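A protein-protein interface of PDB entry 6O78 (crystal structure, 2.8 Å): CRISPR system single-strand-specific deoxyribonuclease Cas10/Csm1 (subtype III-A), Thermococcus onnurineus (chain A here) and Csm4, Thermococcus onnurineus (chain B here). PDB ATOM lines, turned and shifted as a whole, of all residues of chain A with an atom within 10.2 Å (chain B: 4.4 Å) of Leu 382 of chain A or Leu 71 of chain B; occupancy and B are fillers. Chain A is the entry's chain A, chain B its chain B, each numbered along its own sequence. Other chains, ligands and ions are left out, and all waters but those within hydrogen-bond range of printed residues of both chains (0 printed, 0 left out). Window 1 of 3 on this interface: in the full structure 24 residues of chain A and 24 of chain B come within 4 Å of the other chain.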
ATOM      1  N   ASP A 253      29.571  22.080  19.232  1.00  0.00           N
ATOM      2  CA  ASP A 253      28.980  20.747  19.531  1.00  0.00           C
ATOM      3  C   ASP A 253      27.452  20.843  19.454  1.00  0.00           C
ATOM      4  O   ASP A 253      26.881  21.741  20.103  1.00  0.00           O
ATOM      5  CB  ASP A 253      29.413  20.229  20.905  1.00  0.00           C
ATOM      6  CG  ASP A 253      28.921  18.820  21.198  1.00  0.00           C
ATOM      7  OD1 ASP A 253      29.227  17.913  20.396  1.00  0.00           O
ATOM      8  OD2 ASP A 253      28.220  18.643  22.218  1.00  0.00           O
ATOM      9  N   SER A 255      23.805  19.420  20.542  1.00  0.00           N
ATOM     10  CA  SER A 255      23.197  18.773  21.736  1.00  0.00           C
ATOM     11  C   SER A 255      21.723  18.451  21.454  1.00  0.00           C
ATOM     12  O   SER A 255      21.056  19.254  20.771  1.00  0.00           O
ATOM     13  CB  SER A 255      23.369  19.619  22.976  1.00  0.00           C
ATOM     14  OG  SER A 255      22.475  20.721  22.977  1.00  0.00           O
ATOM     15  N   TYR A 344      19.867  21.514  19.322  1.00  0.00           N
ATOM     16  CA  TYR A 344      20.595  22.772  19.631  1.00  0.00           C
ATOM     17  C   TYR A 344      22.019  22.694  19.073  1.00  0.00           C
ATOM     18  O   TYR A 344      22.547  21.576  18.917  1.00  0.00           O
ATOM     19  CB  TYR A 344      20.636  23.000  21.143  1.00  0.00           C
ATOM     20  CG  TYR A 344      21.336  24.264  21.573  1.00  0.00           C
ATOM     21  CD1 TYR A 344      20.933  25.495  21.081  1.00  0.00           C
ATOM     22  CD2 TYR A 344      22.385  24.238  22.480  1.00  0.00           C
ATOM     23  CE1 TYR A 344      21.561  26.666  21.467  1.00  0.00           C
ATOM     24  CE2 TYR A 344      23.019  25.403  22.881  1.00  0.00           C
ATOM     25  CZ  TYR A 344      22.604  26.620  22.372  1.00  0.00           C
ATOM     26  OH  TYR A 344      23.212  27.778  22.753  1.00  0.00           O
ATOM     27  N   LEU A 345      22.616  23.855  18.787  1.00  0.00           N
ATOM     28  CA  LEU A 345      24.048  23.986  18.415  1.00  0.00           C
ATOM     29  C   LEU A 345      24.726  24.975  19.370  1.00  0.00           C
ATOM     30  O   LEU A 345      24.438  26.184  19.280  1.00  0.00           O
ATOM     31  CB  LEU A 345      24.156  24.441  16.956  1.00  0.00           C
ATOM     32  CG  LEU A 345      25.570  24.481  16.378  1.00  0.00           C
ATOM     33  CD1 LEU A 345      26.304  23.165  16.597  1.00  0.00           C
ATOM     34  CD2 LEU A 345      25.535  24.823  14.899  1.00  0.00           C
ATOM     35  N   ALA A 346      25.580  24.456  20.258  1.00  0.00           N
ATOM     36  CA  ALA A 346      26.405  25.229  21.216  1.00  0.00           C
ATOM     37  C   ALA A 346      27.733  25.602  20.547  1.00  0.00           C
ATOM     38  O   ALA A 346      28.601  24.714  20.425  1.00  0.00           O
ATOM     39  CB  ALA A 346      26.626  24.425  22.474  1.00  0.00           C
ATOM     40  N   ILE A 347      27.867  26.859  20.112  1.00  0.00           N
ATOM     41  CA  ILE A 347      29.117  27.424  19.517  1.00  0.00           C
ATOM     42  C   ILE A 347      29.756  28.366  20.542  1.00  0.00           C
ATOM     43  O   ILE A 347      29.086  29.334  20.957  1.00  0.00           O
ATOM     44  CB  ILE A 347      28.829  28.134  18.177  1.00  0.00           C
ATOM     45  CG1 ILE A 347      28.175  27.183  17.169  1.00  0.00           C
ATOM     46  CG2 ILE A 347      30.099  28.771  17.626  1.00  0.00           C
ATOM     47  CD1 ILE A 347      28.007  27.753  15.775  1.00  0.00           C
ATOM     48  N   GLU A 348      31.000  28.078  20.935  1.00  0.00           N
ATOM     49  CA  GLU A 348      31.834  28.936  21.818  1.00  0.00           C
ATOM     50  C   GLU A 348      33.254  28.998  21.247  1.00  0.00           C
ATOM     51  O   GLU A 348      33.640  28.067  20.512  1.00  0.00           O
ATOM     52  CB  GLU A 348      31.826  28.402  23.252  1.00  0.00           C
ATOM     53  CG  GLU A 348      30.595  28.807  24.047  1.00  0.00           C
ATOM     54  CD  GLU A 348      30.473  30.290  24.371  1.00  0.00           C
ATOM     55  OE1 GLU A 348      29.392  30.704  24.838  1.00  0.00           O
ATOM     56  OE2 GLU A 348      31.455  31.031  24.155  1.00  0.00           O
ATOM     57  N   LYS A 374      36.019  23.756  26.551  1.00  0.00           N
ATOM     58  CA  LYS A 374      35.061  22.677  26.918  1.00  0.00           C
ATOM     59  C   LYS A 374      34.112  23.216  27.994  1.00  0.00           C
ATOM     60  O   LYS A 374      32.891  23.036  27.842  1.00  0.00           O
ATOM     61  CB  LYS A 374      35.799  21.426  27.408  1.00  0.00           C
ATOM     62  CG  LYS A 374      34.909  20.303  27.927  1.00  0.00           C
ATOM     63  CD  LYS A 374      34.149  19.562  26.843  1.00  0.00           C
ATOM     64  CE  LYS A 374      32.891  18.882  27.346  1.00  0.00           C
ATOM     65  NZ  LYS A 374      31.675  19.666  27.020  1.00  0.00           N
ATOM     66  N   HIS A 375      34.663  23.863  29.026  1.00  0.00           N
ATOM     67  CA  HIS A 375      33.909  24.499  30.140  1.00  0.00           C
ATOM     68  C   HIS A 375      32.910  25.517  29.575  1.00  0.00           C
ATOM     69  O   HIS A 375      31.740  25.474  29.995  1.00  0.00           O
ATOM     70  CB  HIS A 375      34.872  25.127  31.158  1.00  0.00           C
ATOM     71  CG  HIS A 375      34.190  25.700  32.356  1.00  0.00           C
ATOM     72  ND1 HIS A 375      33.850  27.037  32.443  1.00  0.00           N
ATOM     73  CD2 HIS A 375      33.781  25.127  33.509  1.00  0.00           C
ATOM     74  CE1 HIS A 375      33.262  27.263  33.601  1.00  0.00           C
ATOM     75  NE2 HIS A 375      33.207  26.106  34.274  1.00  0.00           N
ATOM     76  N   LYS A 376      33.350  26.387  28.655  1.00  0.00           N
ATOM     77  CA  LYS A 376      32.485  27.396  27.978  1.00  0.00           C
ATOM     78  C   LYS A 376      31.294  26.690  27.313  1.00  0.00           C
ATOM     79  O   LYS A 376      30.178  27.244  27.376  1.00  0.00           O
ATOM     80  CB  LYS A 376      33.258  28.202  26.927  1.00  0.00           C
ATOM     81  CG  LYS A 376      34.152  29.314  27.460  1.00  0.00           C
ATOM     82  CD  LYS A 376      34.169  30.545  26.571  1.00  0.00           C
ATOM     83  CE  LYS A 376      35.447  31.351  26.670  1.00  0.00           C
ATOM     84  NZ  LYS A 376      35.721  31.798  28.056  1.00  0.00           N
ATOM     85  N   LEU A 377      31.527  25.522  26.701  1.00  0.00           N
ATOM     86  CA  LEU A 377      30.491  24.735  25.975  1.00  0.00           C
ATOM     87  C   LEU A 377      29.467  24.166  26.963  1.00  0.00           C
ATOM     88  O   LEU A 377      28.260  24.288  26.678  1.00  0.00           O
ATOM     89  CB  LEU A 377      31.155  23.615  25.165  1.00  0.00           C
ATOM     90  CG  LEU A 377      31.740  24.030  23.816  1.00  0.00           C
ATOM     91  CD1 LEU A 377      32.657  22.948  23.273  1.00  0.00           C
ATOM     92  CD2 LEU A 377      30.637  24.345  22.816  1.00  0.00           C
ATOM     93  N   THR A 378      29.918  23.572  28.076  1.00  0.00           N
ATOM     94  CA  THR A 378      29.038  22.929  29.094  1.00  0.00           C
ATOM     95  C   THR A 378      28.022  23.959  29.607  1.00  0.00           C
ATOM     96  O   THR A 378      26.864  23.567  29.855  1.00  0.00           O
ATOM     97  CB  THR A 378      29.810  22.331  30.281  1.00  0.00           C
ATOM     98  OG1 THR A 378      30.243  23.400  31.123  1.00  0.00           O
ATOM     99  CG2 THR A 378      30.997  21.479  29.883  1.00  0.00           C
ATOM    100  N   VAL A 379      28.449  25.219  29.756  1.00  0.00           N
ATOM    101  CA  VAL A 379      27.614  26.361  30.235  1.00  0.00           C
ATOM    102  C   VAL A 379      26.624  26.753  29.131  1.00  0.00           C
ATOM    103  O   VAL A 379      25.451  27.013  29.460  1.00  0.00           O
ATOM    104  CB  VAL A 379      28.487  27.561  30.659  1.00  0.00           C
ATOM    105  CG1 VAL A 379      27.651  28.784  31.005  1.00  0.00           C
ATOM    106  CG2 VAL A 379      29.409  27.208  31.818  1.00  0.00           C
ATOM    107  N   ARG A 380      27.086  26.806  27.877  1.00  0.00           N
ATOM    108  CA  ARG A 380      26.269  27.161  26.683  1.00  0.00           C
ATOM    109  C   ARG A 380      25.186  26.092  26.471  1.00  0.00           C
ATOM    110  O   ARG A 380      24.051  26.468  26.114  1.00  0.00           O
ATOM    111  CB  ARG A 380      27.180  27.327  25.460  1.00  0.00           C
ATOM    112  CG  ARG A 380      26.456  27.565  24.143  1.00  0.00           C
ATOM    113  CD  ARG A 380      25.504  28.744  24.169  1.00  0.00           C
ATOM    114  NE  ARG A 380      26.141  30.001  24.531  1.00  0.00           N
ATOM    115  CZ  ARG A 380      25.490  31.124  24.826  1.00  0.00           C
ATOM    116  NH1 ARG A 380      24.166  31.159  24.819  1.00  0.00           N
ATOM    117  NH2 ARG A 380      26.172  32.215  25.130  1.00  0.00           N
ATOM    118  N   LYS A 381      25.516  24.817  26.701  1.00  0.00           N
ATOM    119  CA  LYS A 381      24.561  23.677  26.604  1.00  0.00           C
ATOM    120  C   LYS A 381      23.567  23.724  27.774  1.00  0.00           C
ATOM    121  O   LYS A 381      22.497  23.097  27.651  1.00  0.00           O
ATOM    122  CB  LYS A 381      25.308  22.339  26.583  1.00  0.00           C
ATOM    123  CG  LYS A 381      26.185  22.100  25.362  1.00  0.00           C
ATOM    124  CD  LYS A 381      26.749  20.695  25.300  1.00  0.00           C
ATOM    125  CE  LYS A 381      28.224  20.654  24.964  1.00  0.00           C
ATOM    126  NZ  LYS A 381      28.764  19.276  25.049  1.00  0.00           N
ATOM    127  N   LEU A 382      23.910  24.422  28.866  1.00  0.00           N
ATOM    128  CA  LEU A 382      23.009  24.694  30.022  1.00  0.00           C
ATOM    129  C   LEU A 382      22.295  26.042  29.833  1.00  0.00           C
ATOM    130  O   LEU A 382      21.665  26.515  30.803  1.00  0.00           O
ATOM    131  CB  LEU A 382      23.826  24.683  31.319  1.00  0.00           C
ATOM    132  CG  LEU A 382      24.175  23.300  31.864  1.00  0.00           C
ATOM    133  CD1 LEU A 382      25.309  23.387  32.871  1.00  0.00           C
ATOM    134  CD2 LEU A 382      22.958  22.635  32.489  1.00  0.00           C
ATOM    135  N   LYS A 383      22.393  26.634  28.636  1.00  0.00           N
ATOM    136  CA  LYS A 383      21.696  27.887  28.245  1.00  0.00           C
ATOM    137  C   LYS A 383      21.088  27.685  26.851  1.00  0.00           C
ATOM    138  O   LYS A 383      21.265  28.569  25.987  1.00  0.00           O
ATOM    139  CB  LYS A 383      22.672  29.070  28.302  1.00  0.00           C
ATOM    140  CG  LYS A 383      23.194  29.407  29.695  1.00  0.00           C
ATOM    141  CD  LYS A 383      24.488  30.200  29.702  1.00  0.00           C
ATOM    142  CE  LYS A 383      24.278  31.699  29.721  1.00  0.00           C
ATOM    143  NZ  LYS A 383      23.926  32.187  31.077  1.00  0.00           N
ATOM    144  N   ARG A 384      20.393  26.556  26.656  1.00  0.00           N
ATOM    145  CA  ARG A 384      19.788  26.138  25.361  1.00  0.00           C
ATOM    146  C   ARG A 384      18.832  27.229  24.871  1.00  0.00           C
ATOM    147  O   ARG A 384      17.822  27.477  25.552  1.00  0.00           O
ATOM    148  CB  ARG A 384      19.040  24.807  25.502  1.00  0.00           C
ATOM    149  CG  ARG A 384      19.937  23.608  25.775  1.00  0.00           C
ATOM    150  CD  ARG A 384      19.208  22.285  25.614  1.00  0.00           C
ATOM    151  NE  ARG A 384      18.871  21.991  24.226  1.00  0.00           N
ATOM    152  CZ  ARG A 384      18.305  20.863  23.799  1.00  0.00           C
ATOM    153  NH1 ARG A 384      18.003  19.898  24.652  1.00  0.00           N
ATOM    154  NH2 ARG A 384      18.045  20.702  22.513  1.00  0.00           N
ATOM    155  N   PHE A 385      19.165  27.859  23.740  1.00  0.00           N
ATOM    156  CA  PHE A 385      18.347  28.883  23.038  1.00  0.00           C
ATOM    157  C   PHE A 385      18.231  30.148  23.899  1.00  0.00           C
ATOM    158  O   PHE A 385      17.206  30.854  23.796  1.00  0.00           O
ATOM    159  CB  PHE A 385      16.979  28.309  22.662  1.00  0.00           C
ATOM    160  CG  PHE A 385      17.038  27.101  21.764  1.00  0.00           C
ATOM    161  CD1 PHE A 385      17.300  27.238  20.410  1.00  0.00           C
ATOM    162  CD2 PHE A 385      16.835  25.826  22.270  1.00  0.00           C
ATOM    163  CE1 PHE A 385      17.355  26.129  19.582  1.00  0.00           C
ATOM    164  CE2 PHE A 385      16.891  24.717  21.440  1.00  0.00           C
ATOM    165  CZ  PHE A 385      17.150  24.871  20.098  1.00  0.00           C
ATOM    166  N   GLY A 386      19.263  30.438  24.703  1.00  0.00           N
ATOM    167  CA  GLY A 386      19.432  31.724  25.405  1.00  0.00           C
ATOM    168  C   GLY A 386      19.662  32.861  24.422  1.00  0.00           C
ATOM    169  O   GLY A 386      19.449  34.028  24.808  1.00  0.00           O
ATOM    170  N   GLU A 387      20.067  32.526  23.189  1.00  0.00           N
ATOM    171  CA  GLU A 387      20.292  33.477  22.065  1.00  0.00           C
ATOM    172  C   GLU A 387      18.957  33.809  21.378  1.00  0.00           C
ATOM    173  O   GLU A 387      18.994  34.499  20.340  1.00  0.00           O
ATOM    174  CB  GLU A 387      21.286  32.889  21.058  1.00  0.00           C
ATOM    175  CG  GLU A 387      22.583  32.392  21.679  1.00  0.00           C
ATOM    176  CD  GLU A 387      22.662  30.889  21.903  1.00  0.00           C
ATOM    177  OE1 GLU A 387      23.724  30.305  21.609  1.00  0.00           O
ATOM    178  OE2 GLU A 387      21.663  30.306  22.372  1.00  0.00           O
ATOM    179  N   LEU A 391      11.694  33.346  23.406  1.00  0.00           N
ATOM    180  CA  LEU A 391      11.530  31.986  23.990  1.00  0.00           C
ATOM    181  C   LEU A 391      10.671  32.044  25.260  1.00  0.00           C
ATOM    182  O   LEU A 391       9.764  31.199  25.390  1.00  0.00           O
ATOM    183  CB  LEU A 391      12.920  31.412  24.291  1.00  0.00           C
ATOM    184  CG  LEU A 391      12.954  30.017  24.913  1.00  0.00           C
ATOM    185  CD1 LEU A 391      12.211  29.008  24.050  1.00  0.00           C
ATOM    186  CD2 LEU A 391      14.389  29.565  25.135  1.00  0.00           C
ATOM    187  N   PHE A 392      10.946  33.003  26.153  1.00  0.00           N
ATOM    188  CA  PHE A 392      10.355  33.102  27.515  1.00  0.00           C
ATOM    189  C   PHE A 392       9.201  34.113  27.517  1.00  0.00           C
ATOM    190  O   PHE A 392       9.199  35.023  28.374  1.00  0.00           O
ATOM    191  CB  PHE A 392      11.443  33.465  28.529  1.00  0.00           C
ATOM    192  CG  PHE A 392      12.647  32.556  28.497  1.00  0.00           C
ATOM    193  CD1 PHE A 392      12.508  31.188  28.681  1.00  0.00           C
ATOM    194  CD2 PHE A 392      13.919  33.063  28.280  1.00  0.00           C
ATOM    195  CE1 PHE A 392      13.613  30.351  28.652  1.00  0.00           C
ATOM    196  CE2 PHE A 392      15.023  32.224  28.249  1.00  0.00           C
ATOM    197  CZ  PHE A 392      14.868  30.870  28.437  1.00  0.00           C
ATOM    198  N   LYS B  69      18.715  17.246  41.391  1.00  0.00           N
ATOM    199  CA  LYS B  69      20.105  17.767  41.297  1.00  0.00           C
ATOM    200  C   LYS B  69      20.045  19.194  40.760  1.00  0.00           C
ATOM    201  O   LYS B  69      19.574  19.403  39.644  1.00  0.00           O
ATOM    202  CB  LYS B  69      20.940  16.874  40.375  1.00  0.00           C
ATOM    203  CG  LYS B  69      22.301  17.427  39.967  1.00  0.00           C
ATOM    204  CD  LYS B  69      22.826  16.815  38.685  1.00  0.00           C
ATOM    205  CE  LYS B  69      24.240  17.236  38.348  1.00  0.00           C
ATOM    206  NZ  LYS B  69      25.227  16.634  39.277  1.00  0.00           N
ATOM    207  N   PRO B  70      20.495  20.217  41.522  1.00  0.00           N
ATOM    208  CA  PRO B  70      20.529  21.587  41.011  1.00  0.00           C
ATOM    209  C   PRO B  70      21.581  21.719  39.899  1.00  0.00           C
ATOM    210  O   PRO B  70      22.690  21.267  40.100  1.00  0.00           O
ATOM    211  CB  PRO B  70      20.892  22.433  42.239  1.00  0.00           C
ATOM    212  CG  PRO B  70      21.631  21.475  43.149  1.00  0.00           C
ATOM    213  CD  PRO B  70      20.998  20.120  42.902  1.00  0.00           C
ATOM    214  N   LEU B  71      21.208  22.328  38.768  1.00  0.00           N
ATOM    215  CA  LEU B  71      22.067  22.452  37.558  1.00  0.00           C
ATOM    216  C   LEU B  71      23.306  23.305  37.864  1.00  0.00           C
ATOM    217  O   LEU B  71      24.248  23.267  37.055  1.00  0.00           O
ATOM    218  CB  LEU B  71      21.255  23.071  36.413  1.00  0.00           C
ATOM    219  CG  LEU B  71      20.124  22.217  35.835  1.00  0.00           C
ATOM    220  CD1 LEU B  71      19.605  22.833  34.546  1.00  0.00           C
ATOM    221  CD2 LEU B  71      20.564  20.781  35.587  1.00  0.00           C
ATOM    222  N   SER B  72      23.295  24.043  38.981  1.00  0.00           N
ATOM    223  CA  SER B  72      24.397  24.923  39.460  1.00  0.00           C
ATOM    224  C   SER B  72      25.700  24.134  39.639  1.00  0.00           C
ATOM    225  O   SER B  72      26.775  24.747  39.485  1.00  0.00           O
ATOM    226  CB  SER B  72      24.011  25.610  40.743  1.00  0.00           C
ATOM    227  OG  SER B  72      23.804  24.660  41.778  1.00  0.00           O
ATOM    228  N   VAL B  73      25.618  22.841  39.971  1.00  0.00           N
ATOM    229  CA  VAL B  73      26.810  21.975  40.219  1.00  0.00           C
ATOM    230  C   VAL B  73      27.484  21.659  38.877  1.00  0.00           C
ATOM    231  O   VAL B  73      28.725  21.632  38.850  1.00  0.00           O
ATOM    232  CB  VAL B  73      26.460  20.691  41.001  1.00  0.00           C
ATOM    233  CG1 VAL B  73      25.755  20.998  42.313  1.00  0.00           C
ATOM    234  CG2 VAL B  73      25.646  19.704  40.180  1.00  0.00           C
ATOM    235  N   GLU B  74      26.695  21.487  37.807  1.00  0.00           N
ATOM    236  CA  GLU B  74      27.123  20.942  36.485  1.00  0.00           C
ATOM    237  C   GLU B  74      28.429  21.585  36.010  1.00  0.00           C
ATOM    238  O   GLU B  74      29.361  20.868  35.654  1.00  0.00           O
ATOM    239  CB  GLU B  74      26.016  21.114  35.440  1.00  0.00           C
ATOM    240  CG  GLU B  74      24.772  20.284  35.707  1.00  0.00           C
ATOM    241  CD  GLU B  74      24.801  18.886  35.117  1.00  0.00           C
ATOM    242  OE1 GLU B  74      25.896  18.293  35.064  1.00  0.00           O
ATOM    243  OE2 GLU B  74      23.729  18.397  34.704  1.00  0.00           O
ATOM    244  N   PRO B  75      28.562  22.933  35.957  1.00  0.00           N
ATOM    245  CA  PRO B  75      29.804  23.563  35.506  1.00  0.00           C
ATOM    246  C   PRO B  75      30.898  23.602  36.588  1.00  0.00           C
ATOM    247  O   PRO B  75      32.046  23.822  36.242  1.00  0.00           O
ATOM    248  CB  PRO B  75      29.388  24.998  35.131  1.00  0.00           C
ATOM    249  CG  PRO B  75      27.877  25.040  35.303  1.00  0.00           C
ATOM    250  CD  PRO B  75      27.549  23.943  36.291  1.00  0.00           C
ATOM    251  N   LEU B 226      21.082  29.094  34.636  1.00  0.00           N
ATOM    252  CA  LEU B 226      21.331  27.750  34.048  1.00  0.00           C
ATOM    253  C   LEU B 226      19.987  27.025  33.941  1.00  0.00           C
ATOM    254  O   LEU B 226      19.166  27.192  34.865  1.00  0.00           O
ATOM    255  CB  LEU B 226      22.293  26.965  34.945  1.00  0.00           C
ATOM    256  CG  LEU B 226      23.679  27.578  35.145  1.00  0.00           C
ATOM    257  CD1 LEU B 226      24.477  26.773  36.156  1.00  0.00           C
ATOM    258  CD2 LEU B 226      24.435  27.675  33.828  1.00  0.00           C
ATOM    259  N   TRP B 227      19.764  26.253  32.872  1.00  0.00           N
ATOM    260  CA  TRP B 227      18.464  25.569  32.641  1.00  0.00           C
ATOM    261  C   TRP B 227      18.580  24.433  31.618  1.00  0.00           C
ATOM    262  O   TRP B 227      19.524  24.439  30.805  1.00  0.00           O
ATOM    263  CB  TRP B 227      17.399  26.587  32.219  1.00  0.00           C
ATOM    264  CG  TRP B 227      17.500  27.074  30.805  1.00  0.00           C
ATOM    265  CD1 TRP B 227      16.902  26.526  29.707  1.00  0.00           C
ATOM    266  CD2 TRP B 227      18.209  28.235  30.333  1.00  0.00           C
ATOM    267  NE1 TRP B 227      17.201  27.254  28.587  1.00  0.00           N
ATOM    268  CE2 TRP B 227      17.998  28.311  28.939  1.00  0.00           C
ATOM    269  CE3 TRP B 227      19.008  29.209  30.946  1.00  0.00           C
ATOM    270  CZ2 TRP B 227      18.552  29.325  28.158  1.00  0.00           C
ATOM    271  CZ3 TRP B 227      19.550  30.213  30.173  1.00  0.00           C
ATOM    272  CH2 TRP B 227      19.325  30.267  28.797  1.00  0.00           C
ATOM    273  N   ARG B 228      17.635  23.490  31.699  1.00  0.00           N
ATOM    274  CA  ARG B 228      17.247  22.549  30.617  1.00  0.00           C
ATOM    275  C   ARG B 228      15.793  22.852  30.245  1.00  0.00           C
ATOM    276  O   ARG B 228      14.980  23.033  31.173  1.00  0.00           O
ATOM    277  CB  ARG B 228      17.411  21.094  31.069  1.00  0.00           C
ATOM    278  CG  ARG B 228      18.853  20.691  31.340  1.00  0.00           C
ATOM    279  CD  ARG B 228      19.057  19.188  31.387  1.00  0.00           C
ATOM    280  NE  ARG B 228      20.357  18.839  31.948  1.00  0.00           N
ATOM    281  CZ  ARG B 228      21.523  18.925  31.307  1.00  0.00           C
ATOM    282  NH1 ARG B 228      21.581  19.353  30.056  1.00  0.00           N
ATOM    283  NH2 ARG B 228      22.640  18.581  31.927  1.00  0.00           N
ATOM    284  N   GLY B 250      15.249  21.963  38.882  1.00  0.00           N
ATOM    285  CA  GLY B 250      16.701  22.029  39.142  1.00  0.00           C
ATOM    286  C   GLY B 250      17.370  23.197  38.433  1.00  0.00           C
ATOM    287  O   GLY B 250      18.568  23.424  38.682  1.00  0.00           O
ATOM    288  N   SER B 251      16.637  23.913  37.578  1.00  0.00           N
ATOM    289  CA  SER B 251      17.135  25.095  36.827  1.00  0.00           C
ATOM    290  C   SER B 251      17.319  26.276  37.786  1.00  0.00           C
ATOM    291  O   SER B 251      16.559  26.364  38.772  1.00  0.00           O
ATOM    292  CB  SER B 251      16.208  25.447  35.707  1.00  0.00           C
ATOM    293  OG  SER B 251      16.050  24.353  34.817  1.00  0.00           O
ATOM    294  N   ILE B 252      18.285  27.150  37.490  1.00  0.00           N
ATOM    295  CA  ILE B 252      18.705  28.282  38.369  1.00  0.00           C
ATOM    296  C   ILE B 252      18.092  29.584  37.838  1.00  0.00           C
ATOM    297  O   ILE B 252      18.091  29.787  36.609  1.00  0.00           O
ATOM    298  CB  ILE B 252      20.242  28.355  38.466  1.00  0.00           C
ATOM    299  CG1 ILE B 252      20.864  26.989  38.772  1.00  0.00           C
ATOM    300  CG2 ILE B 252      20.668  29.410  39.474  1.00  0.00           C
ATOM    301  CD1 ILE B 252      20.309  26.310  40.003  1.00  0.00           C
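O of Pro 75 of chain B sits at hydrogen-bond distance from NE2 of His 375 of chain A, at 3.2 Å.
The backbone NH (N) of Trp 227 of chain B lies within hydrogen-bond range of the backbone carbonyl oxygen (O) of Leu 382 of chain A, at 2.8 Å.
NE1 of Trp 227 of chain B lies within hydrogen-bond range of O of Arg 384 of chain A (3.1 Å).
The side-chain carboxylate of Glu 74 of chain B lies within salt-bridge range of the guanidinium group of Arg 228 of chain B.
The backbone NH (N) of Leu 71 of chain B sits at hydrogen-bond distance from the backbone carbonyl oxygen (O) of Gly 250 of chain B (2.9 Å).
O of His 375 of chain A lies within hydrogen-bond range of OG1 of Thr 378 of chain A, 2.8 Å away.
O of Leu 226 of chain B is in hydrogen-bond range of N of Ile 252 of chain B (2.8 Å).
Among the printed residues, merely in contact across the chains: Lys 383 of chain A with Trp 227 of chain B, Leu 382 of chain A with Leu 226 of chain B, Leu 382 of chain A with Glu 74 of chain B, Gly 386 of chain A with Trp 227 of chain B, Leu 382 of chain A with Pro 75 of chain B, Leu 382 of chain A with Leu 71 of chain B and Val 379 of chain A with Pro 75 of chain B.
Ala 346 of chain A touches none of the printed residues of chain B.
Of the printed residues of chain B, His 375 of chain A touches Pro 75.
Of the printed residues of chain B, Val 379 of chain A touches Pro 75 (3.98 Å).
Leu 382 of chain A touches five residues of chain B.
Of the printed residues of chain B, Lys 383 of chain A touches Trp 227 (3.3 Å).
Printed residues of chain B within 4 Å of Arg 384 of chain A: Trp 227.
Leu 391 of chain A touches none of the printed residues of chain B.
No residue of chain A comes within 4 Å of Pro 70 of chain B.
Leu 71 of chain B touches just one residue of chain A: Leu 382.
No residue of chain A comes within 4 Å of Ser 72 of chain B.
Glu 74 of chain B touches one residue of chain A.
Of the printed residues of chain A, Leu 226 of chain B touches Leu 382.
No residue of chain A comes within 4 Å of Arg 228 of chain B.
The nearest residue of chain B that does not touch Leu 382 of chain A is Arg 228 of chain B (4.1 Å).
Of the 13 printed residues of chain B, 5 touch a printed residue of chain A.
Hydrophobic or aromatic side chains of chain B that line the printed part of chain A: Leu 71, Pro 75, Leu 226 and Trp 227.
Of the 23 printed residues of chain A, 6 touch a printed residue of chain B.
Among the printed residues, 10 pairs touch across the chains.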
